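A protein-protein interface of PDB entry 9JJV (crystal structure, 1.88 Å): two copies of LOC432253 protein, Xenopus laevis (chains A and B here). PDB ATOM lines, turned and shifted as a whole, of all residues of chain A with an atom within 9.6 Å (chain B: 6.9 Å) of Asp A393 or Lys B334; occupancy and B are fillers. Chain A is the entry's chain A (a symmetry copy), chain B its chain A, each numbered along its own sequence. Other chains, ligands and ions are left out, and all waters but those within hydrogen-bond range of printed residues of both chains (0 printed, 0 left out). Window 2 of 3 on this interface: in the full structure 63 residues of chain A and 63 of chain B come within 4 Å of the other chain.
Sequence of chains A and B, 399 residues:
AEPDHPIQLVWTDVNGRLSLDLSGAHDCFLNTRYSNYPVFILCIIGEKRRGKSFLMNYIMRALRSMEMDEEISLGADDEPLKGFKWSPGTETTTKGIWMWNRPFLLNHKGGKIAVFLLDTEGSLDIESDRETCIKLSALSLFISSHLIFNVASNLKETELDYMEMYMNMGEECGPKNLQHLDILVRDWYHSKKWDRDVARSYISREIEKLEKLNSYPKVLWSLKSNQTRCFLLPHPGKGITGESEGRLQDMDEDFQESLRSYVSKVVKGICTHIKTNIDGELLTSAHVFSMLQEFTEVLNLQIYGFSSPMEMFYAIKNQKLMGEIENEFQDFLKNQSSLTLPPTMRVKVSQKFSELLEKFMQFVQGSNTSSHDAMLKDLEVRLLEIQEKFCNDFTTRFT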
ATOM      1  N   GLN A 330       1.083  -1.157  14.811  1.00  0.00           N
ATOM      2  CA  GLN A 330       1.012   0.223  14.323  1.00  0.00           C
ATOM      3  C   GLN A 330       0.040   0.365  13.159  1.00  0.00           C
ATOM      4  O   GLN A 330      -0.721   1.332  13.092  1.00  0.00           O
ATOM      5  CB  GLN A 330       2.402   0.692  13.890  1.00  0.00           C
ATOM      6  CG  GLN A 330       3.411   0.735  15.008  1.00  0.00           C
ATOM      7  CD  GLN A 330       3.384   2.052  15.739  1.00  0.00           C
ATOM      8  OE1 GLN A 330       2.370   2.740  15.751  1.00  0.00           O
ATOM      9  NE2 GLN A 330       4.501   2.413  16.355  1.00  0.00           N
ATOM     10  N   LEU A 333      -3.557   0.229  14.385  1.00  0.00           N
ATOM     11  CA  LEU A 333      -3.976   1.481  15.022  1.00  0.00           C
ATOM     12  C   LEU A 333      -4.298   2.559  13.989  1.00  0.00           C
ATOM     13  O   LEU A 333      -5.304   3.273  14.104  1.00  0.00           O
ATOM     14  CB  LEU A 333      -2.876   1.948  15.972  1.00  0.00           C
ATOM     15  CG  LEU A 333      -2.675   1.052  17.196  1.00  0.00           C
ATOM     16  CD1 LEU A 333      -1.711   1.675  18.203  1.00  0.00           C
ATOM     17  CD2 LEU A 333      -4.010   0.842  17.875  1.00  0.00           C
ATOM     18  N   LYS A 334      -3.429   2.712  12.990  1.00  0.00           N
ATOM     19  CA  LYS A 334      -3.635   3.708  11.936  1.00  0.00           C
ATOM     20  C   LYS A 334      -4.924   3.464  11.163  1.00  0.00           C
ATOM     21  O   LYS A 334      -5.582   4.420  10.731  1.00  0.00           O
ATOM     22  CB  LYS A 334      -2.407   3.704  11.017  1.00  0.00           C
ATOM     23  CG  LYS A 334      -2.515   4.473   9.712  1.00  0.00           C
ATOM     24  CD  LYS A 334      -2.927   5.941   9.822  1.00  0.00           C
ATOM     25  CE  LYS A 334      -1.782   6.905   9.503  1.00  0.00           C
ATOM     26  NZ  LYS A 334      -2.033   8.242  10.129  1.00  0.00           N
ATOM     27  N   GLN A 336      -7.691   2.279  12.356  1.00  0.00           N
ATOM     28  CA  GLN A 336      -8.898   2.430  13.155  1.00  0.00           C
ATOM     29  C   GLN A 336      -9.591   3.740  12.810  1.00  0.00           C
ATOM     30  O   GLN A 336      -8.951   4.738  12.469  1.00  0.00           O
ATOM     31  CB  GLN A 336      -8.556   2.382  14.640  1.00  0.00           C
ATOM     32  CG  GLN A 336      -7.983   1.025  15.061  1.00  0.00           C
ATOM     33  CD  GLN A 336      -8.771  -0.142  14.483  1.00  0.00           C
ATOM     34  OE1 GLN A 336      -9.919  -0.354  14.850  1.00  0.00           O
ATOM     35  NE2 GLN A 336      -8.162  -0.889  13.567  1.00  0.00           N
ATOM     36  N   SER A 338     -11.359   7.098  13.609  1.00  0.00           N
ATOM     37  CA  SER A 338     -11.405   8.079  14.685  1.00  0.00           C
ATOM     38  C   SER A 338     -12.823   8.335  15.175  1.00  0.00           C
ATOM     39  O   SER A 338     -13.003   9.083  16.144  1.00  0.00           O
ATOM     40  CB  SER A 338     -10.807   9.406  14.226  1.00  0.00           C
ATOM     41  OG  SER A 338     -11.451   9.857  13.044  1.00  0.00           O
ATOM     42  N   PRO A 342     -14.376   6.060  22.505  1.00  0.00           N
ATOM     43  CA  PRO A 342     -13.123   5.698  23.202  1.00  0.00           C
ATOM     44  C   PRO A 342     -13.208   4.366  23.938  1.00  0.00           C
ATOM     45  O   PRO A 342     -12.262   3.574  23.852  1.00  0.00           O
ATOM     46  CB  PRO A 342     -12.915   6.866  24.176  1.00  0.00           C
ATOM     47  CG  PRO A 342     -13.506   8.051  23.447  1.00  0.00           C
ATOM     48  CD  PRO A 342     -14.712   7.492  22.672  1.00  0.00           C
ATOM     49  N   MET A 345     -13.038   1.582  21.440  1.00  0.00           N
ATOM     50  CA  MET A 345     -11.686   1.554  20.894  1.00  0.00           C
ATOM     51  C   MET A 345     -10.714   0.852  21.835  1.00  0.00           C
ATOM     52  O   MET A 345      -9.895   0.035  21.403  1.00  0.00           O
ATOM     53  CB  MET A 345     -11.196   2.968  20.593  1.00  0.00           C
ATOM     54  CG  MET A 345      -9.760   2.949  20.063  1.00  0.00           C
ATOM     55  SD  MET A 345      -9.689   2.805  18.272  1.00  0.00           S
ATOM     56  CE  MET A 345      -9.945   1.051  18.002  1.00  0.00           C
ATOM     57  N   ARG A 346     -10.786   1.166  23.129  1.00  0.00           N
ATOM     58  CA  ARG A 346      -9.808   0.610  24.055  1.00  0.00           C
ATOM     59  C   ARG A 346      -9.893  -0.911  24.092  1.00  0.00           C
ATOM     60  O   ARG A 346      -8.870  -1.601  24.195  1.00  0.00           O
ATOM     61  CB  ARG A 346     -10.027   1.203  25.442  1.00  0.00           C
ATOM     62  CG  ARG A 346      -8.971   0.816  26.439  1.00  0.00           C
ATOM     63  CD  ARG A 346      -9.182   1.576  27.736  1.00  0.00           C
ATOM     64  NE  ARG A 346      -9.443   2.991  27.519  1.00  0.00           N
ATOM     65  CZ  ARG A 346      -8.535   3.956  27.618  1.00  0.00           C
ATOM     66  NH1 ARG A 346      -7.273   3.688  27.910  1.00  0.00           N
ATOM     67  NH2 ARG A 346      -8.911   5.221  27.431  1.00  0.00           N
ATOM     68  N   ARG A 382       6.951  -2.650  24.685  1.00  0.00           N
ATOM     69  CA  ARG A 382       6.923  -1.756  23.532  1.00  0.00           C
ATOM     70  C   ARG A 382       5.496  -1.560  23.020  1.00  0.00           C
ATOM     71  O   ARG A 382       5.089  -0.427  22.720  1.00  0.00           O
ATOM     72  CB  ARG A 382       7.827  -2.283  22.417  1.00  0.00           C
ATOM     73  CG  ARG A 382       7.696  -1.497  21.106  1.00  0.00           C
ATOM     74  CD  ARG A 382       7.988   0.013  21.298  1.00  0.00           C
ATOM     75  NE  ARG A 382       8.034   0.749  20.035  1.00  0.00           N
ATOM     76  CZ  ARG A 382       7.712   2.034  19.896  1.00  0.00           C
ATOM     77  NH1 ARG A 382       7.350   2.776  20.935  1.00  0.00           N
ATOM     78  NH2 ARG A 382       7.746   2.588  18.684  1.00  0.00           N
ATOM     79  N   GLU A 385       3.640   0.865  25.311  1.00  0.00           N
ATOM     80  CA  GLU A 385       3.893   2.272  25.004  1.00  0.00           C
ATOM     81  C   GLU A 385       3.039   2.728  23.835  1.00  0.00           C
ATOM     82  O   GLU A 385       2.421   3.794  23.878  1.00  0.00           O
ATOM     83  CB  GLU A 385       5.358   2.526  24.673  1.00  0.00           C
ATOM     84  CG  GLU A 385       6.389   2.053  25.652  1.00  0.00           C
ATOM     85  CD  GLU A 385       7.793   2.295  25.103  1.00  0.00           C
ATOM     86  OE1 GLU A 385       8.607   1.345  25.062  1.00  0.00           O
ATOM     87  OE2 GLU A 385       8.065   3.443  24.676  1.00  0.00           O
ATOM     88  N   ILE A 386       3.025   1.935  22.764  1.00  0.00           N
ATOM     89  CA  ILE A 386       2.254   2.288  21.580  1.00  0.00           C
ATOM     90  C   ILE A 386       0.785   2.411  21.939  1.00  0.00           C
ATOM     91  O   ILE A 386       0.110   3.357  21.528  1.00  0.00           O
ATOM     92  CB  ILE A 386       2.489   1.249  20.467  1.00  0.00           C
ATOM     93  CG1 ILE A 386       3.976   1.148  20.136  1.00  0.00           C
ATOM     94  CG2 ILE A 386       1.738   1.623  19.201  1.00  0.00           C
ATOM     95  CD1 ILE A 386       4.268   0.115  19.062  1.00  0.00           C
ATOM     96  N   GLN A 387       0.286   1.483  22.754  1.00  0.00           N
ATOM     97  CA  GLN A 387      -1.124   1.495  23.143  1.00  0.00           C
ATOM     98  C   GLN A 387      -1.464   2.726  23.974  1.00  0.00           C
ATOM     99  O   GLN A 387      -2.455   3.417  23.712  1.00  0.00           O
ATOM    100  CB  GLN A 387      -1.433   0.226  23.932  1.00  0.00           C
ATOM    101  CG  GLN A 387      -2.889   0.016  24.277  1.00  0.00           C
ATOM    102  CD  GLN A 387      -3.061  -1.263  25.063  1.00  0.00           C
ATOM    103  OE1 GLN A 387      -3.727  -2.196  24.618  1.00  0.00           O
ATOM    104  NE2 GLN A 387      -2.458  -1.314  26.247  1.00  0.00           N
ATOM    105  N   GLU A 388      -0.654   2.996  24.999  1.00  0.00           N
ATOM    106  CA  GLU A 388      -0.873   4.137  25.887  1.00  0.00           C
ATOM    107  C   GLU A 388      -0.970   5.442  25.109  1.00  0.00           C
ATOM    108  O   GLU A 388      -1.928   6.209  25.264  1.00  0.00           O
ATOM    109  CB  GLU A 388       0.279   4.205  26.888  1.00  0.00           C
ATOM    110  CG  GLU A 388      -0.044   3.790  28.300  1.00  0.00           C
ATOM    111  CD  GLU A 388       0.899   4.449  29.293  1.00  0.00           C
ATOM    112  OE1 GLU A 388       0.783   4.181  30.509  1.00  0.00           O
ATOM    113  OE2 GLU A 388       1.780   5.220  28.842  1.00  0.00           O
ATOM    114  N   LYS A 389       0.036   5.709  24.275  1.00  0.00           N
ATOM    115  CA  LYS A 389       0.056   6.909  23.451  1.00  0.00           C
ATOM    116  C   LYS A 389      -1.194   7.007  22.591  1.00  0.00           C
ATOM    117  O   LYS A 389      -1.807   8.074  22.483  1.00  0.00           O
ATOM    118  CB  LYS A 389       1.302   6.893  22.568  1.00  0.00           C
ATOM    119  CG  LYS A 389       1.605   8.215  21.899  1.00  0.00           C
ATOM    120  CD  LYS A 389       3.074   8.259  21.534  1.00  0.00           C
ATOM    121  CE  LYS A 389       3.541   9.687  21.371  1.00  0.00           C
ATOM    122  NZ  LYS A 389       5.031   9.737  21.278  1.00  0.00           N
ATOM    123  N   PHE A 390      -1.584   5.896  21.964  1.00  0.00           N
ATOM    124  CA  PHE A 390      -2.761   5.917  21.104  1.00  0.00           C
ATOM    125  C   PHE A 390      -4.020   6.183  21.918  1.00  0.00           C
ATOM    126  O   PHE A 390      -4.805   7.079  21.587  1.00  0.00           O
ATOM    127  CB  PHE A 390      -2.881   4.597  20.334  1.00  0.00           C
ATOM    128  CG  PHE A 390      -4.063   4.545  19.404  1.00  0.00           C
ATOM    129  CD1 PHE A 390      -5.302   4.093  19.842  1.00  0.00           C
ATOM    130  CD2 PHE A 390      -3.937   4.968  18.084  1.00  0.00           C
ATOM    131  CE1 PHE A 390      -6.396   4.053  18.984  1.00  0.00           C
ATOM    132  CE2 PHE A 390      -5.036   4.941  17.221  1.00  0.00           C
ATOM    133  CZ  PHE A 390      -6.263   4.479  17.673  1.00  0.00           C
ATOM    134  N   CYS A 391      -4.218   5.432  23.007  1.00  0.00           N
ATOM    135  CA  CYS A 391      -5.465   5.554  23.765  1.00  0.00           C
ATOM    136  C   CYS A 391      -5.548   6.838  24.582  1.00  0.00           C
ATOM    137  O   CYS A 391      -6.653   7.228  24.968  1.00  0.00           O
ATOM    138  CB  CYS A 391      -5.654   4.354  24.690  1.00  0.00           C
ATOM    139  SG  CYS A 391      -6.070   2.811  23.816  1.00  0.00           S
ATOM    140  N   ASN A 392      -4.426   7.496  24.879  1.00  0.00           N
ATOM    141  CA  ASN A 392      -4.518   8.804  25.528  1.00  0.00           C
ATOM    142  C   ASN A 392      -4.882   9.888  24.525  1.00  0.00           C
ATOM    143  O   ASN A 392      -5.675  10.787  24.831  1.00  0.00           O
ATOM    144  CB  ASN A 392      -3.203   9.172  26.217  1.00  0.00           C
ATOM    145  CG  ASN A 392      -2.885   8.284  27.399  1.00  0.00           C
ATOM    146  OD1 ASN A 392      -3.524   7.251  27.611  1.00  0.00           O
ATOM    147  ND2 ASN A 392      -1.885   8.682  28.183  1.00  0.00           N
ATOM    148  N   ASP A 393      -4.301   9.824  23.328  1.00  0.00           N
ATOM    149  CA  ASP A 393      -4.554  10.835  22.315  1.00  0.00           C
ATOM    150  C   ASP A 393      -5.895  10.628  21.627  1.00  0.00           C
ATOM    151  O   ASP A 393      -6.477  11.593  21.120  1.00  0.00           O
ATOM    152  CB  ASP A 393      -3.410  10.833  21.292  1.00  0.00           C
ATOM    153  CG  ASP A 393      -3.517  11.964  20.279  1.00  0.00           C
ATOM    154  OD1 ASP A 393      -3.720  13.130  20.700  1.00  0.00           O
ATOM    155  OD2 ASP A 393      -3.369  11.692  19.064  1.00  0.00           O
ATOM    156  N   PHE A 394      -6.408   9.401  21.626  1.00  0.00           N
ATOM    157  CA  PHE A 394      -7.666   9.110  20.962  1.00  0.00           C
ATOM    158  C   PHE A 394      -8.826   9.731  21.747  1.00  0.00           C
ATOM    159  O   PHE A 394      -9.615  10.506  21.206  1.00  0.00           O
ATOM    160  CB  PHE A 394      -7.879   7.594  20.806  1.00  0.00           C
ATOM    161  CG  PHE A 394      -9.054   7.246  19.936  1.00  0.00           C
ATOM    162  CD1 PHE A 394     -10.336   7.201  20.466  1.00  0.00           C
ATOM    163  CD2 PHE A 394      -8.879   6.973  18.582  1.00  0.00           C
ATOM    164  CE1 PHE A 394     -11.429   6.915  19.666  1.00  0.00           C
ATOM    165  CE2 PHE A 394      -9.973   6.663  17.773  1.00  0.00           C
ATOM    166  CZ  PHE A 394     -11.249   6.635  18.320  1.00  0.00           C
ATOM    167  N   PHE B 329      10.500   7.098  13.216  1.00  0.00           N
ATOM    168  CA  PHE B 329       9.619   7.746  12.249  1.00  0.00           C
ATOM    169  C   PHE B 329       8.182   7.720  12.735  1.00  0.00           C
ATOM    170  O   PHE B 329       7.497   8.751  12.741  1.00  0.00           O
ATOM    171  CB  PHE B 329       9.745   7.063  10.883  1.00  0.00           C
ATOM    172  CG  PHE B 329       9.254   7.902   9.737  1.00  0.00           C
ATOM    173  CD1 PHE B 329       9.575   9.246   9.655  1.00  0.00           C
ATOM    174  CD2 PHE B 329       8.459   7.343   8.743  1.00  0.00           C
ATOM    175  CE1 PHE B 329       9.121  10.023   8.591  1.00  0.00           C
ATOM    176  CE2 PHE B 329       8.008   8.102   7.688  1.00  0.00           C
ATOM    177  CZ  PHE B 329       8.328   9.452   7.614  1.00  0.00           C
ATOM    178  N   GLN B 330       7.716   6.545  13.169  1.00  0.00           N
ATOM    179  CA  GLN B 330       6.342   6.411  13.659  1.00  0.00           C
ATOM    180  C   GLN B 330       6.060   7.349  14.826  1.00  0.00           C
ATOM    181  O   GLN B 330       4.991   7.959  14.895  1.00  0.00           O
ATOM    182  CB  GLN B 330       6.085   4.966  14.090  1.00  0.00           C
ATOM    183  CG  GLN B 330       6.189   3.963  12.971  1.00  0.00           C
ATOM    184  CD  GLN B 330       4.881   3.797  12.242  1.00  0.00           C
ATOM    185  OE1 GLN B 330       4.051   4.698  12.234  1.00  0.00           O
ATOM    186  NE2 GLN B 330       4.688   2.639  11.625  1.00  0.00           N
ATOM    187  N   ASP B 331       6.994   7.456  15.774  1.00  0.00           N
ATOM    188  CA  ASP B 331       6.781   8.342  16.917  1.00  0.00           C
ATOM    189  C   ASP B 331       6.727   9.792  16.467  1.00  0.00           C
ATOM    190  O   ASP B 331       5.908  10.579  16.961  1.00  0.00           O
ATOM    191  CB  ASP B 331       7.896   8.152  17.951  1.00  0.00           C
ATOM    192  CG  ASP B 331       7.861   6.776  18.624  1.00  0.00           C
ATOM    193  OD1 ASP B 331       7.095   5.891  18.170  1.00  0.00           O
ATOM    194  OD2 ASP B 331       8.653   6.563  19.575  1.00  0.00           O
ATOM    195  N   PHE B 332       7.596  10.166  15.525  1.00  0.00           N
ATOM    196  CA  PHE B 332       7.574  11.526  15.006  1.00  0.00           C
ATOM    197  C   PHE B 332       6.225  11.860  14.384  1.00  0.00           C
ATOM    198  O   PHE B 332       5.684  12.949  14.610  1.00  0.00           O
ATOM    199  CB  PHE B 332       8.697  11.705  13.993  1.00  0.00           C
ATOM    200  CG  PHE B 332       8.622  12.978  13.225  1.00  0.00           C
ATOM    201  CD1 PHE B 332       9.236  14.122  13.705  1.00  0.00           C
ATOM    202  CD2 PHE B 332       7.977  13.029  12.000  1.00  0.00           C
ATOM    203  CE1 PHE B 332       9.178  15.306  12.994  1.00  0.00           C
ATOM    204  CE2 PHE B 332       7.925  14.196  11.290  1.00  0.00           C
ATOM    205  CZ  PHE B 332       8.529  15.336  11.781  1.00  0.00           C
ATOM    206  N   LEU B 333       5.660  10.929  13.606  1.00  0.00           N
ATOM    207  CA  LEU B 333       4.360  11.160  12.971  1.00  0.00           C
ATOM    208  C   LEU B 333       3.248  11.317  14.006  1.00  0.00           C
ATOM    209  O   LEU B 333       2.392  12.206  13.895  1.00  0.00           O
ATOM    210  CB  LEU B 333       4.058  10.004  12.020  1.00  0.00           C
ATOM    211  CG  LEU B 333       4.972   9.939  10.795  1.00  0.00           C
ATOM    212  CD1 LEU B 333       4.497   8.895   9.787  1.00  0.00           C
ATOM    213  CD2 LEU B 333       4.981  11.292  10.117  1.00  0.00           C
ATOM    214  N   LYS B 334       3.226  10.433  15.005  1.00  0.00           N
ATOM    215  CA  LYS B 334       2.212  10.488  16.059  1.00  0.00           C
ATOM    216  C   LYS B 334       2.265  11.798  16.834  1.00  0.00           C
ATOM    217  O   LYS B 334       1.223  12.306  17.270  1.00  0.00           O
ATOM    218  CB  LYS B 334       2.400   9.272  16.977  1.00  0.00           C
ATOM    219  CG  LYS B 334       1.626   9.263  18.283  1.00  0.00           C
ATOM    220  CD  LYS B 334       0.113   9.453  18.177  1.00  0.00           C
ATOM    221  CE  LYS B 334      -0.671   8.179  18.495  1.00  0.00           C
ATOM    222  NZ  LYS B 334      -2.031   8.230  17.872  1.00  0.00           N
ATOM    223  N   ASN B 335       3.458  12.364  16.998  1.00  0.00           N
ATOM    224  CA  ASN B 335       3.663  13.595  17.735  1.00  0.00           C
ATOM    225  C   ASN B 335       3.309  14.840  16.935  1.00  0.00           C
ATOM    226  O   ASN B 335       3.279  15.933  17.513  1.00  0.00           O
ATOM    227  CB  ASN B 335       5.115  13.685  18.194  1.00  0.00           C
ATOM    228  CG  ASN B 335       5.431  12.696  19.293  1.00  0.00           C
ATOM    229  OD1 ASN B 335       4.536  12.253  20.020  1.00  0.00           O
ATOM    230  ND2 ASN B 335       6.700  12.342  19.417  1.00  0.00           N
ATOM    231  N   GLN B 336       3.026  14.711  15.645  1.00  0.00           N
ATOM    232  CA  GLN B 336       2.696  15.884  14.849  1.00  0.00           C
ATOM    233  C   GLN B 336       1.298  16.375  15.197  1.00  0.00           C
ATOM    234  O   GLN B 336       0.407  15.593  15.539  1.00  0.00           O
ATOM    235  CB  GLN B 336       2.792  15.555  13.363  1.00  0.00           C
ATOM    236  CG  GLN B 336       4.217  15.189  12.939  1.00  0.00           C
ATOM    237  CD  GLN B 336       5.256  16.141  13.517  1.00  0.00           C
ATOM    238  OE1 GLN B 336       5.296  17.307  13.151  1.00  0.00           O
ATOM    239  NE2 GLN B 336       6.087  15.647  14.430  1.00  0.00           N
ATOM    240  N   SER B 337       1.120  17.691  15.137  1.00  0.00           N
ATOM    241  CA  SER B 337      -0.175  18.290  15.402  1.00  0.00           C
ATOM    242  C   SER B 337      -1.081  18.156  14.190  1.00  0.00           C
ATOM    243  O   SER B 337      -0.716  18.568  13.087  1.00  0.00           O
ATOM    244  CB  SER B 337      -0.019  19.764  15.773  1.00  0.00           C
ATOM    245  OG  SER B 337      -1.297  20.359  15.845  1.00  0.00           O
ATOM    246  N   PHE B 390       0.334   8.151   6.032  1.00  0.00           N
ATOM    247  CA  PHE B 390       0.141   9.311   6.894  1.00  0.00           C
ATOM    248  C   PHE B 390      -0.310  10.518   6.083  1.00  0.00           C
ATOM    249  O   PHE B 390      -1.312  11.161   6.417  1.00  0.00           O
ATOM    250  CB  PHE B 390       1.430   9.624   7.662  1.00  0.00           C
ATOM    251  CG  PHE B 390       1.308  10.798   8.595  1.00  0.00           C
ATOM    252  CD1 PHE B 390       1.571  12.092   8.158  1.00  0.00           C
ATOM    253  CD2 PHE B 390       0.911  10.609   9.915  1.00  0.00           C
ATOM    254  CE1 PHE B 390       1.450  13.178   9.018  1.00  0.00           C
ATOM    255  CE2 PHE B 390       0.777  11.699  10.779  1.00  0.00           C
ATOM    256  CZ  PHE B 390       1.051  12.982  10.330  1.00  0.00           C
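Of the 10 printed residues of chain B, 5 touch a printed residue of chain A.
Printed residues of chain B that touch a printed residue of chain A: Gln B330, Asp B331, Lys B334, Asn B335 and Phe B390.
Printed residues of chain A that touch a printed residue of chain B: Gln A330, Lys A334, Arg A382, Lys A389, Phe A390 and Asp A393.
Hydrophobic or aromatic side chains of chain A within 4 Å of the printed part of chain B: Phe A390.
Among the printed residues, Asp or Glu carboxylates within 4 Å of a Lys or Arg side-chain nitrogen of the other chain: Arg A382 with Asp B331 (3.4 Å) and Asp A393 with Lys B334 (3.9 Å).
Lys B334 touches just these residues of chain A: Lys A389 (3.7 Å), Phe A390 (3.8 Å) and Asp A393 (3.9 Å).
Printed residues of chain A within 4 Å of Phe B390: Lys A334.
Printed residues of chain B within 4 Å of Arg A382: Asp B331 (3.4 Å).
Printed residues of chain B within 4 Å of Lys A334: Phe B390.
Of the printed residues of chain B, Lys A389 touches Lys B334 (3.7 Å) and Asn B335 (2.9 Å).
Of the printed residues of chain B, Gln A330 touches Gln B330 (3.8 Å).
The nearest residue of chain A that does not touch Lys B334 is Ile A386 (5.7 Å).
The nearest printed residue of chain B that does not touch Lys A389 is Asp B331 (4.5 Å).
The side-chain carboxylate of Asp B331 is in salt-bridge range of the guanidinium group of Arg A382, 3.4 Å away.
The side-chain carboxylate (OD2) of Asp A393 is in salt-bridge range of the side-chain amino group (NZ) of Lys B334, 3.9 Å away.
The side-chain amide oxygen (OD1) of Asn B335 lies within hydrogen-bond range of the side-chain amino group (NZ) of Lys A389, 2.9 Å away.
Gln B330 touches its own counterpart, Gln A330.
Lys A334 touches Phe B390, and with the chains exchanged Phe A390 touches Lys B334.
5 positions are printed for both chains.
NE2 of Gln B330 touches CB of Gln A330, at 3.8 Å.
Phe B390 touches Lys A334.
CG of Lys B334 touches CE of Lys A389, 3.7 Å away.
Phe A390 touches Lys B334 (CD2 to NZ, 3.8 Å).
ND2 of Asn B335 sits at hydrogen-bond distance from O of Asp B331 (3.1 Å).
NH1 of Arg A382 is in salt-bridge range of OE2 of Glu A385, at 3.9 Å.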
